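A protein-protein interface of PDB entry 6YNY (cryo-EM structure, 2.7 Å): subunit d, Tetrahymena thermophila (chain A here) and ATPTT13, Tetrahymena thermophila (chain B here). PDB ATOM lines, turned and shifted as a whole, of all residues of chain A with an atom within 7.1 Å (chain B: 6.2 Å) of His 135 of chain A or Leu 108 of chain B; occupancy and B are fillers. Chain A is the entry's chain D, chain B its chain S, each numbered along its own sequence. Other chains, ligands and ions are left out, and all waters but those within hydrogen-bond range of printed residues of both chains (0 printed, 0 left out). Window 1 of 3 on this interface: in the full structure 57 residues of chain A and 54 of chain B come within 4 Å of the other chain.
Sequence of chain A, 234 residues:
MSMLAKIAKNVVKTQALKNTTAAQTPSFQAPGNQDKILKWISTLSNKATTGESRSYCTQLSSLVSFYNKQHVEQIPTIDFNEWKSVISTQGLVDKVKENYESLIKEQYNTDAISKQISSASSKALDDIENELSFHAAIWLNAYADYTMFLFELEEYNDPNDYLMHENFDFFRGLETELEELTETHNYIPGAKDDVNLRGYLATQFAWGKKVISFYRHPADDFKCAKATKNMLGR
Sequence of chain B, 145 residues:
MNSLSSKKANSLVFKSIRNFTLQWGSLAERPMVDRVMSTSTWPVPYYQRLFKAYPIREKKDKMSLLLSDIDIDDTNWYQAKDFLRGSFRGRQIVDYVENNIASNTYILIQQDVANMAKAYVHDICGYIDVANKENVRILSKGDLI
O of Leu 108 of chain B sits at hydrogen-bond distance from NE1 of Trp 139 of chain A.
Val 97 of chain B touches Asn 130 of chain A (CG2 to O, 3.0 Å). Glu 131 of chain A touches Ile 101 of chain B. O of Glu 131 of chain A touches CD1 of Leu 108 of chain B, 3.8 Å away. CB of Phe 134 of chain A touches CG2 of Val 97 of chain B (3.8 Å). O of Tyr 106 of chain B touches CE2 of Phe 134 of chain A, 3.9 Å away. Phe 134 of chain A touches Leu 108 of chain B (CD2 to CD1, 3.9 Å). Leu 108 of chain B touches His 135 of chain A (O to CD2, 3.1 Å). Gln 110 of chain B touches His 135 of chain A. Ile 138 of chain A touches Tyr 106 of chain B (CD1 to O, 3.1 Å). Leu 108 of chain B touches Ile 138 of chain A.
Printed residues of chain B within 4 Å of Phe 134 of chain A: Val 97, Tyr 106 and Leu 108. Of chain B, only Leu 108 and Gln 110 come within 4 Å of His 135 of chain A. Of the printed residues of chain B, Ile 138 of chain A touches Tyr 106 (3.1 Å) and Leu 108 (3.97 Å). Leu 140 of chain A touches none of the printed residues of chain B. Of the printed residues of chain A, Val 97 of chain B touches Asn 130 (3.0 Å) and Phe 134 (3.8 Å). Of the printed residues of chain A, Ile 101 of chain B touches Glu 131 (3.6 Å). Printed residues of chain A within 4 Å of Leu 108 of chain B: Glu 131 (3.8 Å), Phe 134 (3.9 Å), His 135 (3.1 Å), Ile 138 (3.97 Å) and Trp 139 (3.1 Å). Printed residues of chain A within 4 Å of Gln 110 of chain B: His 135 (3.5 Å). The nearest residue of chain B that does not touch His 135 of chain A is Ile 109 of chain B (4.1 Å). The nearest printed residue of chain B that does not touch Ile 138 of chain A is Ile 107 of chain B (4.7 Å).
Hydrophobic or aromatic side chains of chain B that line the printed part of chain A: Val 97, Ile 101 and Leu 108. Of the 11 printed residues of chain A, 6 touch a printed residue of chain B. Printed residues of chain A that touch a printed residue of chain B: Asn 130, Glu 131, Phe 134, His 135, Ile 138 and Trp 139. Hydrophobic or aromatic side chains of chain A within 4 Å of the printed part of chain B: Phe 134, His 135, Ile 138 and Trp 139. Among the printed residues, 11 pairs touch across the chains. Among the printed residues, no Asp or Glu carboxylate lies within 4 Å of a Lys or Arg side-chain nitrogen of the other chain.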
ATOM      1  N   ASN A 130       8.894  -0.386 -17.635  1.00  0.00           N
ATOM      2  CA  ASN A 130      10.246  -0.718 -18.048  1.00  0.00           C
ATOM      3  C   ASN A 130      10.407  -0.743 -19.558  1.00  0.00           C
ATOM      4  O   ASN A 130      11.539  -0.684 -20.048  1.00  0.00           O
ATOM      5  CB  ASN A 130      10.652  -2.074 -17.470  1.00  0.00           C
ATOM      6  CG  ASN A 130      10.743  -2.055 -15.963  1.00  0.00           C
ATOM      7  OD1 ASN A 130      11.007  -1.019 -15.359  1.00  0.00           O
ATOM      8  ND2 ASN A 130      10.526  -3.206 -15.347  1.00  0.00           N
ATOM      9  N   GLU A 131       9.306  -0.842 -20.302  1.00  0.00           N
ATOM     10  CA  GLU A 131       9.378  -0.780 -21.755  1.00  0.00           C
ATOM     11  C   GLU A 131       9.530   0.660 -22.228  1.00  0.00           C
ATOM     12  O   GLU A 131      10.421   0.972 -23.024  1.00  0.00           O
ATOM     13  CB  GLU A 131       8.130  -1.415 -22.365  1.00  0.00           C
ATOM     14  CG  GLU A 131       8.196  -1.611 -23.867  1.00  0.00           C
ATOM     15  CD  GLU A 131       6.969  -2.306 -24.420  1.00  0.00           C
ATOM     16  OE1 GLU A 131       6.114  -2.734 -23.617  1.00  0.00           O
ATOM     17  OE2 GLU A 131       6.860  -2.425 -25.658  1.00  0.00           O
ATOM     18  N   LEU A 132       8.664   1.550 -21.742  1.00  0.00           N
ATOM     19  CA  LEU A 132       8.758   2.955 -22.112  1.00  0.00           C
ATOM     20  C   LEU A 132      10.014   3.601 -21.549  1.00  0.00           C
ATOM     21  O   LEU A 132      10.518   4.575 -22.119  1.00  0.00           O
ATOM     22  CB  LEU A 132       7.521   3.706 -21.630  1.00  0.00           C
ATOM     23  CG  LEU A 132       6.190   3.247 -22.216  1.00  0.00           C
ATOM     24  CD1 LEU A 132       5.061   4.037 -21.608  1.00  0.00           C
ATOM     25  CD2 LEU A 132       6.181   3.395 -23.720  1.00  0.00           C
ATOM     26  N   SER A 133      10.528   3.086 -20.433  1.00  0.00           N
ATOM     27  CA  SER A 133      11.758   3.629 -19.874  1.00  0.00           C
ATOM     28  C   SER A 133      12.949   3.310 -20.765  1.00  0.00           C
ATOM     29  O   SER A 133      13.822   4.158 -20.972  1.00  0.00           O
ATOM     30  CB  SER A 133      11.982   3.080 -18.469  1.00  0.00           C
ATOM     31  OG  SER A 133      10.919   3.433 -17.608  1.00  0.00           O
ATOM     32  N   PHE A 134      13.001   2.091 -21.301  1.00  0.00           N
ATOM     33  CA  PHE A 134      14.064   1.745 -22.233  1.00  0.00           C
ATOM     34  C   PHE A 134      13.823   2.386 -23.590  1.00  0.00           C
ATOM     35  O   PHE A 134      14.771   2.803 -24.263  1.00  0.00           O
ATOM     36  CB  PHE A 134      14.162   0.229 -22.363  1.00  0.00           C
ATOM     37  CG  PHE A 134      15.324  -0.233 -23.184  1.00  0.00           C
ATOM     38  CD1 PHE A 134      16.611  -0.150 -22.691  1.00  0.00           C
ATOM     39  CD2 PHE A 134      15.131  -0.760 -24.444  1.00  0.00           C
ATOM     40  CE1 PHE A 134      17.677  -0.576 -23.443  1.00  0.00           C
ATOM     41  CE2 PHE A 134      16.196  -1.187 -25.194  1.00  0.00           C
ATOM     42  CZ  PHE A 134      17.468  -1.094 -24.695  1.00  0.00           C
ATOM     43  N   HIS A 135      12.560   2.479 -24.003  1.00  0.00           N
ATOM     44  CA  HIS A 135      12.235   3.178 -25.238  1.00  0.00           C
ATOM     45  C   HIS A 135      12.667   4.637 -25.177  1.00  0.00           C
ATOM     46  O   HIS A 135      13.180   5.181 -26.160  1.00  0.00           O
ATOM     47  CB  HIS A 135      10.738   3.069 -25.509  1.00  0.00           C
ATOM     48  CG  HIS A 135      10.239   4.015 -26.552  1.00  0.00           C
ATOM     49  ND1 HIS A 135       9.731   5.258 -26.246  1.00  0.00           N
ATOM     50  CD2 HIS A 135      10.162   3.898 -27.897  1.00  0.00           C
ATOM     51  CE1 HIS A 135       9.368   5.868 -27.358  1.00  0.00           C
ATOM     52  NE2 HIS A 135       9.619   5.064 -28.374  1.00  0.00           N
ATOM     53  N   ALA A 136      12.472   5.287 -24.030  1.00  0.00           N
ATOM     54  CA  ALA A 136      12.880   6.680 -23.903  1.00  0.00           C
ATOM     55  C   ALA A 136      14.395   6.809 -23.864  1.00  0.00           C
ATOM     56  O   ALA A 136      14.958   7.760 -24.417  1.00  0.00           O
ATOM     57  CB  ALA A 136      12.259   7.294 -22.654  1.00  0.00           C
ATOM     58  N   ALA A 137      15.072   5.861 -23.215  1.00  0.00           N
ATOM     59  CA  ALA A 137      16.527   5.900 -23.159  1.00  0.00           C
ATOM     60  C   ALA A 137      17.143   5.770 -24.543  1.00  0.00           C
ATOM     61  O   ALA A 137      18.222   6.314 -24.797  1.00  0.00           O
ATOM     62  CB  ALA A 137      17.038   4.796 -22.245  1.00  0.00           C
ATOM     63  N   ILE A 138      16.480   5.050 -25.443  1.00  0.00           N
ATOM     64  CA  ILE A 138      16.970   4.926 -26.809  1.00  0.00           C
ATOM     65  C   ILE A 138      16.929   6.277 -27.509  1.00  0.00           C
ATOM     66  O   ILE A 138      17.903   6.699 -28.141  1.00  0.00           O
ATOM     67  CB  ILE A 138      16.147   3.877 -27.573  1.00  0.00           C
ATOM     68  CG1 ILE A 138      16.359   2.493 -26.972  1.00  0.00           C
ATOM     69  CG2 ILE A 138      16.516   3.873 -29.033  1.00  0.00           C
ATOM     70  CD1 ILE A 138      15.365   1.488 -27.456  1.00  0.00           C
ATOM     71  N   TRP A 139      15.798   6.969 -27.412  1.00  0.00           N
ATOM     72  CA  TRP A 139      15.623   8.237 -28.098  1.00  0.00           C
ATOM     73  C   TRP A 139      16.198   9.411 -27.324  1.00  0.00           C
ATOM     74  O   TRP A 139      16.314  10.504 -27.886  1.00  0.00           O
ATOM     75  CB  TRP A 139      14.140   8.451 -28.385  1.00  0.00           C
ATOM     76  CG  TRP A 139      13.614   7.444 -29.342  1.00  0.00           C
ATOM     77  CD1 TRP A 139      13.092   6.229 -29.040  1.00  0.00           C
ATOM     78  CD2 TRP A 139      13.574   7.554 -30.767  1.00  0.00           C
ATOM     79  NE1 TRP A 139      12.725   5.572 -30.182  1.00  0.00           N
ATOM     80  CE2 TRP A 139      13.010   6.366 -31.260  1.00  0.00           C
ATOM     81  CE3 TRP A 139      13.959   8.543 -31.674  1.00  0.00           C
ATOM     82  CZ2 TRP A 139      12.819   6.141 -32.614  1.00  0.00           C
ATOM     83  CZ3 TRP A 139      13.769   8.316 -33.013  1.00  0.00           C
ATOM     84  CH2 TRP A 139      13.205   7.126 -33.474  1.00  0.00           C
ATOM     85  N   LEU A 140      16.549   9.218 -26.055  1.00  0.00           N
ATOM     86  CA  LEU A 140      17.362  10.201 -25.355  1.00  0.00           C
ATOM     87  C   LEU A 140      18.820  10.104 -25.770  1.00  0.00           C
ATOM     88  O   LEU A 140      19.526  11.118 -25.794  1.00  0.00           O
ATOM     89  CB  LEU A 140      17.236  10.013 -23.847  1.00  0.00           C
ATOM     90  CG  LEU A 140      15.925  10.469 -23.215  1.00  0.00           C
ATOM     91  CD1 LEU A 140      15.841   9.977 -21.795  1.00  0.00           C
ATOM     92  CD2 LEU A 140      15.807  11.975 -23.259  1.00  0.00           C
ATOM     93  N   VAL B  97      13.653  -5.767 -19.721  1.00  0.00           N
ATOM     94  CA  VAL B  97      13.302  -5.557 -21.120  1.00  0.00           C
ATOM     95  C   VAL B  97      13.832  -6.692 -21.984  1.00  0.00           C
ATOM     96  O   VAL B  97      13.142  -7.176 -22.888  1.00  0.00           O
ATOM     97  CB  VAL B  97      13.825  -4.195 -21.599  1.00  0.00           C
ATOM     98  CG1 VAL B  97      13.718  -4.089 -23.100  1.00  0.00           C
ATOM     99  CG2 VAL B  97      13.059  -3.071 -20.943  1.00  0.00           C
ATOM    100  N   ILE B 101       9.824  -8.915 -22.416  1.00  0.00           N
ATOM    101  CA  ILE B 101       9.140  -8.066 -23.385  1.00  0.00           C
ATOM    102  C   ILE B 101       9.191  -8.755 -24.741  1.00  0.00           C
ATOM    103  O   ILE B 101      10.277  -8.997 -25.278  1.00  0.00           O
ATOM    104  CB  ILE B 101       9.752  -6.658 -23.467  1.00  0.00           C
ATOM    105  CG1 ILE B 101       9.380  -5.873 -22.210  1.00  0.00           C
ATOM    106  CG2 ILE B 101       9.274  -5.949 -24.719  1.00  0.00           C
ATOM    107  CD1 ILE B 101       9.932  -4.484 -22.157  1.00  0.00           C
ATOM    108  N   SER B 103       9.255  -8.628 -28.211  1.00  0.00           N
ATOM    109  CA  SER B 103       9.526  -7.744 -29.331  1.00  0.00           C
ATOM    110  C   SER B 103      10.613  -8.359 -30.195  1.00  0.00           C
ATOM    111  O   SER B 103      11.547  -8.981 -29.683  1.00  0.00           O
ATOM    112  CB  SER B 103       9.953  -6.354 -28.854  1.00  0.00           C
ATOM    113  OG  SER B 103      10.040  -5.450 -29.937  1.00  0.00           O
ATOM    114  N   THR B 105      12.800  -6.791 -31.865  1.00  0.00           N
ATOM    115  CA  THR B 105      13.923  -5.881 -32.013  1.00  0.00           C
ATOM    116  C   THR B 105      14.004  -4.994 -30.784  1.00  0.00           C
ATOM    117  O   THR B 105      12.997  -4.746 -30.115  1.00  0.00           O
ATOM    118  CB  THR B 105      13.783  -5.021 -33.273  1.00  0.00           C
ATOM    119  OG1 THR B 105      14.951  -4.209 -33.438  1.00  0.00           O
ATOM    120  CG2 THR B 105      12.564  -4.130 -33.172  1.00  0.00           C
ATOM    121  N   TYR B 106      15.213  -4.523 -30.495  1.00  0.00           N
ATOM    122  CA  TYR B 106      15.440  -3.567 -29.423  1.00  0.00           C
ATOM    123  C   TYR B 106      15.249  -2.128 -29.871  1.00  0.00           C
ATOM    124  O   TYR B 106      15.337  -1.220 -29.039  1.00  0.00           O
ATOM    125  CB  TYR B 106      16.846  -3.728 -28.854  1.00  0.00           C
ATOM    126  CG  TYR B 106      17.017  -4.915 -27.947  1.00  0.00           C
ATOM    127  CD1 TYR B 106      16.339  -4.993 -26.744  1.00  0.00           C
ATOM    128  CD2 TYR B 106      17.878  -5.944 -28.279  1.00  0.00           C
ATOM    129  CE1 TYR B 106      16.496  -6.069 -25.911  1.00  0.00           C
ATOM    130  CE2 TYR B 106      18.046  -7.022 -27.449  1.00  0.00           C
ATOM    131  CZ  TYR B 106      17.351  -7.084 -26.266  1.00  0.00           C
ATOM    132  OH  TYR B 106      17.515  -8.164 -25.435  1.00  0.00           O
ATOM    133  N   ILE B 107      14.990  -1.896 -31.155  1.00  0.00           N
ATOM    134  CA  ILE B 107      14.738  -0.549 -31.660  1.00  0.00           C
ATOM    135  C   ILE B 107      13.247  -0.309 -31.461  1.00  0.00           C
ATOM    136  O   ILE B 107      12.429  -0.514 -32.355  1.00  0.00           O
ATOM    137  CB  ILE B 107      15.164  -0.392 -33.115  1.00  0.00           C
ATOM    138  CG1 ILE B 107      16.601  -0.876 -33.302  1.00  0.00           C
ATOM    139  CG2 ILE B 107      15.036   1.058 -33.539  1.00  0.00           C
ATOM    140  CD1 ILE B 107      17.093  -0.800 -34.718  1.00  0.00           C
ATOM    141  N   LEU B 108      12.897   0.134 -30.260  1.00  0.00           N
ATOM    142  CA  LEU B 108      11.507   0.334 -29.895  1.00  0.00           C
ATOM    143  C   LEU B 108      10.986   1.626 -30.503  1.00  0.00           C
ATOM    144  O   LEU B 108      11.588   2.691 -30.336  1.00  0.00           O
ATOM    145  CB  LEU B 108      11.362   0.357 -28.377  1.00  0.00           C
ATOM    146  CG  LEU B 108      11.901  -0.889 -27.684  1.00  0.00           C
ATOM    147  CD1 LEU B 108      11.692  -0.800 -26.196  1.00  0.00           C
ATOM    148  CD2 LEU B 108      11.242  -2.125 -28.239  1.00  0.00           C
ATOM    149  N   ILE B 109       9.866   1.527 -31.210  1.00  0.00           N
ATOM    150  CA  ILE B 109       9.242   2.661 -31.871  1.00  0.00           C
ATOM    151  C   ILE B 109       7.772   2.658 -31.490  1.00  0.00           C
ATOM    152  O   ILE B 109       7.043   1.716 -31.823  1.00  0.00           O
ATOM    153  CB  ILE B 109       9.407   2.604 -33.396  1.00  0.00           C
ATOM    154  CG1 ILE B 109      10.880   2.427 -33.755  1.00  0.00           C
ATOM    155  CG2 ILE B 109       8.874   3.865 -34.028  1.00  0.00           C
ATOM    156  CD1 ILE B 109      11.145   2.338 -35.231  1.00  0.00           C
ATOM    157  N   GLN B 110       7.341   3.701 -30.790  1.00  0.00           N
ATOM    158  CA  GLN B 110       5.960   3.823 -30.344  1.00  0.00           C
ATOM    159  C   GLN B 110       5.177   4.589 -31.402  1.00  0.00           C
ATOM    160  O   GLN B 110       5.411   5.781 -31.619  1.00  0.00           O
ATOM    161  CB  GLN B 110       5.889   4.519 -28.989  1.00  0.00           C
ATOM    162  CG  GLN B 110       6.415   3.684 -27.840  1.00  0.00           C
ATOM    163  CD  GLN B 110       5.629   2.410 -27.632  1.00  0.00           C
ATOM    164  OE1 GLN B 110       6.200   1.325 -27.532  1.00  0.00           O
ATOM    165  NE2 GLN B 110       4.312   2.535 -27.557  1.00  0.00           N
